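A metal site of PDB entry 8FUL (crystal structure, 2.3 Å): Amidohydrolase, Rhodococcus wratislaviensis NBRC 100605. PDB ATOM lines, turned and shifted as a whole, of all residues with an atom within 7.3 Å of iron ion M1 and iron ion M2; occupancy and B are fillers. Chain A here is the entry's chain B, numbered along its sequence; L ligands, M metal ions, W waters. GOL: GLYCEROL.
The side-chain amide oxygen (OE1) of Gln 106 sits close to the side-chain carboxylate (OD1) of Asp 25 (3.0 Å).
The side-chain carboxylate (OE2) of Glu 265 lies close to the side-chain amide oxygen (OE1) of Gln 309, 3.4 Å away.
OG of Ser 307 sits at hydrogen-bond distance from N of Glu 265 (3.2 Å).
A ring nitrogen (ND1) of His 27 sits at hydrogen-bond distance from the backbone carbonyl oxygen (O) of Gln 106, at 2.9 Å.
The backbone carbonyl oxygen (O) of Tyr 338 sits at hydrogen-bond distance from the backbone NH (N) of His 27, at 2.8 Å.
The side-chain carboxylate (OD2) of Asp 337 sits close to the side-chain amide nitrogen (NE2) of Gln 309 (2.9 Å).
Within 4 Å of iron ion M2: Glu 265, Asp 337 and His 340.
The nearest printed residue that does not touch iron ion M1 is His 340 (4.4 Å).
OD2 of Asp 25 is bound to iron ion M1 (1.9 Å).
Iron ion M1 is bound by the side-chain carboxylate (OE1) of Glu 265 (2.0 Å).
NE2 of His 27 binds iron ion M1 (2.1 Å).
Water W1 is bound to iron ion M1, at 2.1 Å.
Iron ion M1 is bound by NE2 of His 211 (2.3 Å).
Iron ion M1 is bound by the side-chain carboxylate (OD1) of Asp 337, 2.3 Å away.
ND1 of His 340 binds iron ion M2 (2.1 Å).
Iron ion M2 is bound by O1 of the ligand (2.2 Å).
Iron ion M2 is bound by the side-chain carboxylate (OE2) of Glu 265 (2.2 Å).
Water W1 is bound to iron ion M2.
The side-chain carboxylate (OD2) of Asp 337 binds iron ion M2, 2.3 Å away.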
ATOM      1  N   ALA A  24      20.990  -6.341   0.342  1.00  0.00           N
ATOM      2  CA  ALA A  24      21.920  -7.090   1.162  1.00  0.00           C
ATOM      3  C   ALA A  24      22.604  -6.242   2.220  1.00  0.00           C
ATOM      4  O   ALA A  24      23.405  -6.780   3.001  1.00  0.00           O
ATOM      5  CB  ALA A  24      22.981  -7.756   0.287  1.00  0.00           C
ATOM      6  N   ASP A  25      22.331  -4.945   2.287  1.00  0.00           N
ATOM      7  CA  ASP A  25      23.023  -4.116   3.273  1.00  0.00           C
ATOM      8  C   ASP A  25      22.079  -3.012   3.747  1.00  0.00           C
ATOM      9  O   ASP A  25      21.961  -1.980   3.086  1.00  0.00           O
ATOM     10  CB  ASP A  25      24.318  -3.535   2.717  1.00  0.00           C
ATOM     11  CG  ASP A  25      25.244  -3.056   3.822  1.00  0.00           C
ATOM     12  OD1 ASP A  25      25.015  -3.436   4.994  1.00  0.00           O
ATOM     13  OD2 ASP A  25      26.192  -2.300   3.543  1.00  0.00           O
ATOM     14  N   ILE A  26      21.481  -3.226   4.914  1.00  0.00           N
ATOM     15  CA  ILE A  26      20.724  -2.202   5.628  1.00  0.00           C
ATOM     16  C   ILE A  26      21.398  -1.973   6.974  1.00  0.00           C
ATOM     17  O   ILE A  26      21.827  -2.942   7.622  1.00  0.00           O
ATOM     18  CB  ILE A  26      19.252  -2.629   5.791  1.00  0.00           C
ATOM     19  CG1 ILE A  26      18.657  -2.984   4.412  1.00  0.00           C
ATOM     20  CG2 ILE A  26      18.449  -1.547   6.452  1.00  0.00           C
ATOM     21  CD1 ILE A  26      17.250  -3.524   4.437  1.00  0.00           C
ATOM     22  N   HIS A  27      21.506  -0.715   7.408  1.00  0.00           N
ATOM     23  CA  HIS A  27      22.218  -0.358   8.638  1.00  0.00           C
ATOM     24  C   HIS A  27      21.281   0.268   9.658  1.00  0.00           C
ATOM     25  O   HIS A  27      21.199   1.493   9.773  1.00  0.00           O
ATOM     26  CB  HIS A  27      23.373   0.615   8.383  1.00  0.00           C
ATOM     27  CG  HIS A  27      24.486   0.028   7.590  1.00  0.00           C
ATOM     28  ND1 HIS A  27      25.032  -1.203   7.872  1.00  0.00           N
ATOM     29  CD2 HIS A  27      25.160   0.507   6.518  1.00  0.00           C
ATOM     30  CE1 HIS A  27      25.994  -1.469   7.006  1.00  0.00           C
ATOM     31  NE2 HIS A  27      26.089  -0.446   6.173  1.00  0.00           N
ATOM     32  N   ALA A  71      28.369  11.305   7.101  1.00  0.00           N
ATOM     33  CA  ALA A  71      28.208  10.418   5.938  1.00  0.00           C
ATOM     34  C   ALA A  71      26.831   9.747   5.900  1.00  0.00           C
ATOM     35  O   ALA A  71      26.654   8.692   5.270  1.00  0.00           O
ATOM     36  CB  ALA A  71      29.314   9.360   5.891  1.00  0.00           C
ATOM     37  N   GLN A 106      22.602  -5.344   8.836  1.00  0.00           N
ATOM     38  CA  GLN A 106      24.016  -5.411   9.232  1.00  0.00           C
ATOM     39  C   GLN A 106      24.265  -4.337  10.279  1.00  0.00           C
ATOM     40  O   GLN A 106      24.671  -3.214   9.932  1.00  0.00           O
ATOM     41  CB  GLN A 106      24.921  -5.242   8.039  1.00  0.00           C
ATOM     42  CG  GLN A 106      24.517  -6.144   6.932  1.00  0.00           C
ATOM     43  CD  GLN A 106      25.630  -6.407   5.998  1.00  0.00           C
ATOM     44  OE1 GLN A 106      26.649  -5.720   6.005  1.00  0.00           O
ATOM     45  NE2 GLN A 106      25.463  -7.433   5.177  1.00  0.00           N
ATOM     46  N   LEU A 108      26.260  -2.351  12.672  1.00  0.00           N
ATOM     47  CA  LEU A 108      27.676  -2.040  12.819  1.00  0.00           C
ATOM     48  C   LEU A 108      27.968  -1.090  13.974  1.00  0.00           C
ATOM     49  O   LEU A 108      29.054  -0.518  14.015  1.00  0.00           O
ATOM     50  CB  LEU A 108      28.238  -1.417  11.543  1.00  0.00           C
ATOM     51  CG  LEU A 108      28.041  -1.976  10.129  1.00  0.00           C
ATOM     52  CD1 LEU A 108      28.805  -1.073   9.160  1.00  0.00           C
ATOM     53  CD2 LEU A 108      28.472  -3.427  10.005  1.00  0.00           C
ATOM     54  N   THR A 114      28.287   5.668  12.898  1.00  0.00           N
ATOM     55  CA  THR A 114      28.293   5.074  11.566  1.00  0.00           C
ATOM     56  C   THR A 114      28.998   3.706  11.515  1.00  0.00           C
ATOM     57  O   THR A 114      28.476   2.757  10.915  1.00  0.00           O
ATOM     58  CB  THR A 114      28.969   6.035  10.573  1.00  0.00           C
ATOM     59  OG1 THR A 114      28.153   7.195  10.365  1.00  0.00           O
ATOM     60  CG2 THR A 114      29.266   5.348   9.230  1.00  0.00           C
ATOM     61  N   HIS A 211      31.518  -7.159   5.780  1.00  0.00           N
ATOM     62  CA  HIS A 211      31.185  -5.777   5.490  1.00  0.00           C
ATOM     63  C   HIS A 211      32.394  -4.866   5.705  1.00  0.00           C
ATOM     64  O   HIS A 211      33.176  -5.075   6.630  1.00  0.00           O
ATOM     65  CB  HIS A 211      30.042  -5.312   6.379  1.00  0.00           C
ATOM     66  CG  HIS A 211      29.550  -3.939   6.059  1.00  0.00           C
ATOM     67  ND1 HIS A 211      30.206  -2.793   6.465  1.00  0.00           N
ATOM     68  CD2 HIS A 211      28.470  -3.517   5.346  1.00  0.00           C
ATOM     69  CE1 HIS A 211      29.561  -1.726   6.024  1.00  0.00           C
ATOM     70  NE2 HIS A 211      28.507  -2.138   5.346  1.00  0.00           N
ATOM     71  N   LEU A 212      32.517  -3.873   4.843  1.00  0.00           N
ATOM     72  CA  LEU A 212      33.518  -2.823   4.955  1.00  0.00           C
ATOM     73  C   LEU A 212      33.715  -2.411   6.400  1.00  0.00           C
ATOM     74  O   LEU A 212      32.740  -2.240   7.140  1.00  0.00           O
ATOM     75  CB  LEU A 212      33.077  -1.621   4.105  1.00  0.00           C
ATOM     76  CG  LEU A 212      33.633  -0.206   4.179  1.00  0.00           C
ATOM     77  CD1 LEU A 212      33.460   0.425   2.814  1.00  0.00           C
ATOM     78  CD2 LEU A 212      32.960   0.671   5.261  1.00  0.00           C
ATOM     79  N   HIS A 233      38.454   6.155   1.742  1.00  0.00           N
ATOM     80  CA  HIS A 233      37.244   5.529   1.240  1.00  0.00           C
ATOM     81  C   HIS A 233      37.528   4.673   0.010  1.00  0.00           C
ATOM     82  O   HIS A 233      37.114   3.507  -0.044  1.00  0.00           O
ATOM     83  CB  HIS A 233      36.177   6.595   0.978  1.00  0.00           C
ATOM     84  CG  HIS A 233      34.794   6.040   0.878  1.00  0.00           C
ATOM     85  ND1 HIS A 233      33.684   6.831   0.668  1.00  0.00           N
ATOM     86  CD2 HIS A 233      34.331   4.765   0.918  1.00  0.00           C
ATOM     87  CE1 HIS A 233      32.612   6.072   0.591  1.00  0.00           C
ATOM     88  NE2 HIS A 233      32.974   4.809   0.743  1.00  0.00           N
ATOM     89  N   VAL A 264      30.754  -7.371   1.211  1.00  0.00           N
ATOM     90  CA  VAL A 264      29.726  -6.331   1.245  1.00  0.00           C
ATOM     91  C   VAL A 264      30.379  -4.949   1.286  1.00  0.00           C
ATOM     92  O   VAL A 264      31.151  -4.653   2.213  1.00  0.00           O
ATOM     93  CB  VAL A 264      28.754  -6.512   2.421  1.00  0.00           C
ATOM     94  CG1 VAL A 264      27.749  -5.396   2.407  1.00  0.00           C
ATOM     95  CG2 VAL A 264      28.046  -7.852   2.318  1.00  0.00           C
ATOM     96  N   GLU A 265      30.039  -4.113   0.310  1.00  0.00           N
ATOM     97  CA  GLU A 265      30.439  -2.707   0.251  1.00  0.00           C
ATOM     98  C   GLU A 265      31.937  -2.558  -0.039  1.00  0.00           C
ATOM     99  O   GLU A 265      32.603  -1.679   0.489  1.00  0.00           O
ATOM    100  CB  GLU A 265      30.028  -1.932   1.520  1.00  0.00           C
ATOM    101  CG  GLU A 265      30.091  -0.437   1.342  1.00  0.00           C
ATOM    102  CD  GLU A 265      29.277   0.320   2.332  1.00  0.00           C
ATOM    103  OE1 GLU A 265      28.465  -0.314   3.027  1.00  0.00           O
ATOM    104  OE2 GLU A 265      29.436   1.568   2.402  1.00  0.00           O
ATOM    105  N   SER A 307      28.113  -7.682  -3.013  1.00  0.00           N
ATOM    106  CA  SER A 307      27.039  -6.712  -3.134  1.00  0.00           C
ATOM    107  C   SER A 307      27.520  -5.522  -3.971  1.00  0.00           C
ATOM    108  O   SER A 307      28.704  -5.380  -4.253  1.00  0.00           O
ATOM    109  CB  SER A 307      26.544  -6.281  -1.755  1.00  0.00           C
ATOM    110  OG  SER A 307      27.416  -5.331  -1.171  1.00  0.00           O
ATOM    111  N   GLN A 309      26.488  -1.819  -3.814  1.00  0.00           N
ATOM    112  CA  GLN A 309      26.747  -0.505  -3.280  1.00  0.00           C
ATOM    113  C   GLN A 309      28.203  -0.382  -2.828  1.00  0.00           C
ATOM    114  O   GLN A 309      28.751  -1.313  -2.225  1.00  0.00           O
ATOM    115  CB  GLN A 309      25.791  -0.224  -2.106  1.00  0.00           C
ATOM    116  CG  GLN A 309      25.685   1.264  -1.691  1.00  0.00           C
ATOM    117  CD  GLN A 309      26.785   1.669  -0.737  1.00  0.00           C
ATOM    118  OE1 GLN A 309      27.514   0.815  -0.257  1.00  0.00           O
ATOM    119  NE2 GLN A 309      26.868   2.938  -0.417  1.00  0.00           N
ATOM    120  N   PRO A 310      28.883   0.743  -3.125  1.00  0.00           N
ATOM    121  CA  PRO A 310      28.394   1.812  -4.012  1.00  0.00           C
ATOM    122  C   PRO A 310      28.661   1.442  -5.470  1.00  0.00           C
ATOM    123  O   PRO A 310      29.798   1.111  -5.789  1.00  0.00           O
ATOM    124  CB  PRO A 310      29.220   3.025  -3.594  1.00  0.00           C
ATOM    125  CG  PRO A 310      30.492   2.470  -3.068  1.00  0.00           C
ATOM    126  CD  PRO A 310      30.194   1.068  -2.528  1.00  0.00           C
ATOM    127  N   ALA A 335      22.390  -4.038  -3.260  1.00  0.00           N
ATOM    128  CA  ALA A 335      22.268  -3.464  -1.921  1.00  0.00           C
ATOM    129  C   ALA A 335      22.091  -1.961  -2.016  1.00  0.00           C
ATOM    130  O   ALA A 335      22.588  -1.317  -2.955  1.00  0.00           O
ATOM    131  CB  ALA A 335      23.480  -3.826  -1.044  1.00  0.00           C
ATOM    132  N   THR A 336      21.387  -1.384  -1.044  1.00  0.00           N
ATOM    133  CA  THR A 336      21.199   0.053  -0.974  1.00  0.00           C
ATOM    134  C   THR A 336      22.180   0.756  -0.039  1.00  0.00           C
ATOM    135  O   THR A 336      22.505   1.912  -0.273  1.00  0.00           O
ATOM    136  CB  THR A 336      19.790   0.412  -0.493  1.00  0.00           C
ATOM    137  OG1 THR A 336      19.609   0.005   0.866  1.00  0.00           O
ATOM    138  CG2 THR A 336      18.707  -0.194  -1.387  1.00  0.00           C
ATOM    139  N   ASP A 337      22.577   0.101   1.045  1.00  0.00           N
ATOM    140  CA  ASP A 337      23.347   0.747   2.104  1.00  0.00           C
ATOM    141  C   ASP A 337      22.531   1.837   2.792  1.00  0.00           C
ATOM    142  O   ASP A 337      23.048   2.878   3.201  1.00  0.00           O
ATOM    143  CB  ASP A 337      24.654   1.330   1.558  1.00  0.00           C
ATOM    144  CG  ASP A 337      25.659   1.562   2.634  1.00  0.00           C
ATOM    145  OD1 ASP A 337      25.591   0.837   3.639  1.00  0.00           O
ATOM    146  OD2 ASP A 337      26.502   2.470   2.470  1.00  0.00           O
ATOM    147  N   TYR A 338      21.247   1.610   2.939  1.00  0.00           N
ATOM    148  CA  TYR A 338      20.449   2.557   3.700  1.00  0.00           C
ATOM    149  C   TYR A 338      20.922   2.578   5.144  1.00  0.00           C
ATOM    150  O   TYR A 338      21.063   1.515   5.760  1.00  0.00           O
ATOM    151  CB  TYR A 338      18.967   2.196   3.603  1.00  0.00           C
ATOM    152  CG  TYR A 338      18.097   3.135   4.395  1.00  0.00           C
ATOM    153  CD1 TYR A 338      17.653   4.323   3.845  1.00  0.00           C
ATOM    154  CD2 TYR A 338      17.746   2.837   5.710  1.00  0.00           C
ATOM    155  CE1 TYR A 338      16.868   5.190   4.568  1.00  0.00           C
ATOM    156  CE2 TYR A 338      16.971   3.699   6.454  1.00  0.00           C
ATOM    157  CZ  TYR A 338      16.530   4.872   5.881  1.00  0.00           C
ATOM    158  OH  TYR A 338      15.751   5.733   6.609  1.00  0.00           O
ATOM    159  N   PRO A 339      21.158   3.762   5.755  1.00  0.00           N
ATOM    160  CA  PRO A 339      20.908   5.119   5.261  1.00  0.00           C
ATOM    161  C   PRO A 339      22.156   5.951   4.959  1.00  0.00           C
ATOM    162  O   PRO A 339      22.125   7.164   5.157  1.00  0.00           O
ATOM    163  CB  PRO A 339      20.155   5.743   6.427  1.00  0.00           C
ATOM    164  CG  PRO A 339      20.936   5.207   7.625  1.00  0.00           C
ATOM    165  CD  PRO A 339      21.431   3.802   7.212  1.00  0.00           C
ATOM    166  N   HIS A 340      23.251   5.339   4.507  1.00  0.00           N
ATOM    167  CA  HIS A 340      24.481   6.093   4.324  1.00  0.00           C
ATOM    168  C   HIS A 340      24.358   7.043   3.109  1.00  0.00           C
ATOM    169  O   HIS A 340      23.444   6.940   2.291  1.00  0.00           O
ATOM    170  CB  HIS A 340      25.661   5.137   4.166  1.00  0.00           C
ATOM    171  CG  HIS A 340      26.034   4.416   5.429  1.00  0.00           C
ATOM    172  ND1 HIS A 340      27.031   3.480   5.483  1.00  0.00           N
ATOM    173  CD2 HIS A 340      25.533   4.511   6.683  1.00  0.00           C
ATOM    174  CE1 HIS A 340      27.132   3.007   6.717  1.00  0.00           C
ATOM    175  NE2 HIS A 340      26.231   3.622   7.466  1.00  0.00           N
ATOM    176  N   PHE A 341      25.322   7.968   3.008  1.00  0.00           N
ATOM    177  CA  PHE A 341      25.169   9.094   2.092  1.00  0.00           C
ATOM    178  C   PHE A 341      25.259   8.652   0.642  1.00  0.00           C
ATOM    179  O   PHE A 341      24.612   9.262  -0.220  1.00  0.00           O
ATOM    180  CB  PHE A 341      26.217  10.179   2.374  1.00  0.00           C
ATOM    181  CG  PHE A 341      27.562   9.959   1.688  1.00  0.00           C
ATOM    182  CD1 PHE A 341      28.576   9.251   2.328  1.00  0.00           C
ATOM    183  CD2 PHE A 341      27.802  10.496   0.429  1.00  0.00           C
ATOM    184  CE1 PHE A 341      29.819   9.073   1.712  1.00  0.00           C
ATOM    185  CE2 PHE A 341      29.047  10.311  -0.199  1.00  0.00           C
ATOM    186  CZ  PHE A 341      30.055   9.603   0.449  1.00  0.00           C
ATOM    187  N   ASP A 342      26.060   7.640   0.346  1.00  0.00           N
ATOM    188  CA  ASP A 342      26.168   7.107  -1.005  1.00  0.00           C
ATOM    189  C   ASP A 342      25.179   5.969  -1.262  1.00  0.00           C
ATOM    190  O   ASP A 342      25.456   5.059  -2.062  1.00  0.00           O
ATOM    191  CB  ASP A 342      27.616   6.686  -1.293  1.00  0.00           C
ATOM    192  CG  ASP A 342      28.173   5.715  -0.259  1.00  0.00           C
ATOM    193  OD1 ASP A 342      27.650   5.681   0.874  1.00  0.00           O
ATOM    194  OD2 ASP A 342      29.125   4.971  -0.580  1.00  0.00           O
ATOM    195  N   PHE A 343      24.030   6.008  -0.574  1.00  0.00           N
ATOM    196  CA  PHE A 343      22.886   5.140  -0.827  1.00  0.00           C
ATOM    197  C   PHE A 343      22.628   4.963  -2.318  1.00  0.00           C
ATOM    198  O   PHE A 343      22.716   5.905  -3.090  1.00  0.00           O
ATOM    199  CB  PHE A 343      21.659   5.750  -0.132  1.00  0.00           C
ATOM    200  CG  PHE A 343      20.336   5.241  -0.615  1.00  0.00           C
ATOM    201  CD1 PHE A 343      19.692   4.216   0.064  1.00  0.00           C
ATOM    202  CD2 PHE A 343      19.700   5.820  -1.704  1.00  0.00           C
ATOM    203  CE1 PHE A 343      18.449   3.757  -0.365  1.00  0.00           C
ATOM    204  CE2 PHE A 343      18.475   5.368  -2.145  1.00  0.00           C
ATOM    205  CZ  PHE A 343      17.845   4.329  -1.480  1.00  0.00           C
HETATM  206  C1  GOL L   1      30.254   5.034   2.978  1.00  0.00           C
HETATM  207  O1  GOL L   1      28.916   4.597   2.821  1.00  0.00           O
HETATM  208  C2  GOL L   1      30.619   5.026   4.487  1.00  0.00           C
HETATM  209  O2  GOL L   1      29.551   5.430   5.273  1.00  0.00           O
HETATM  210  C3  GOL L   1      30.980   3.556   4.831  1.00  0.00           C
HETATM  211  O3  GOL L   1      30.764   3.393   6.244  1.00  0.00           O
HETATM  212 FE    FE M   1      26.976  -0.814   4.336  1.00  0.00          FE
HETATM  213 FE    FE M   2      28.291   2.792   3.884  1.00  0.00          FE
HETATM  214  O   HOH W   1      28.199   0.799   4.936  1.00  0.00           O
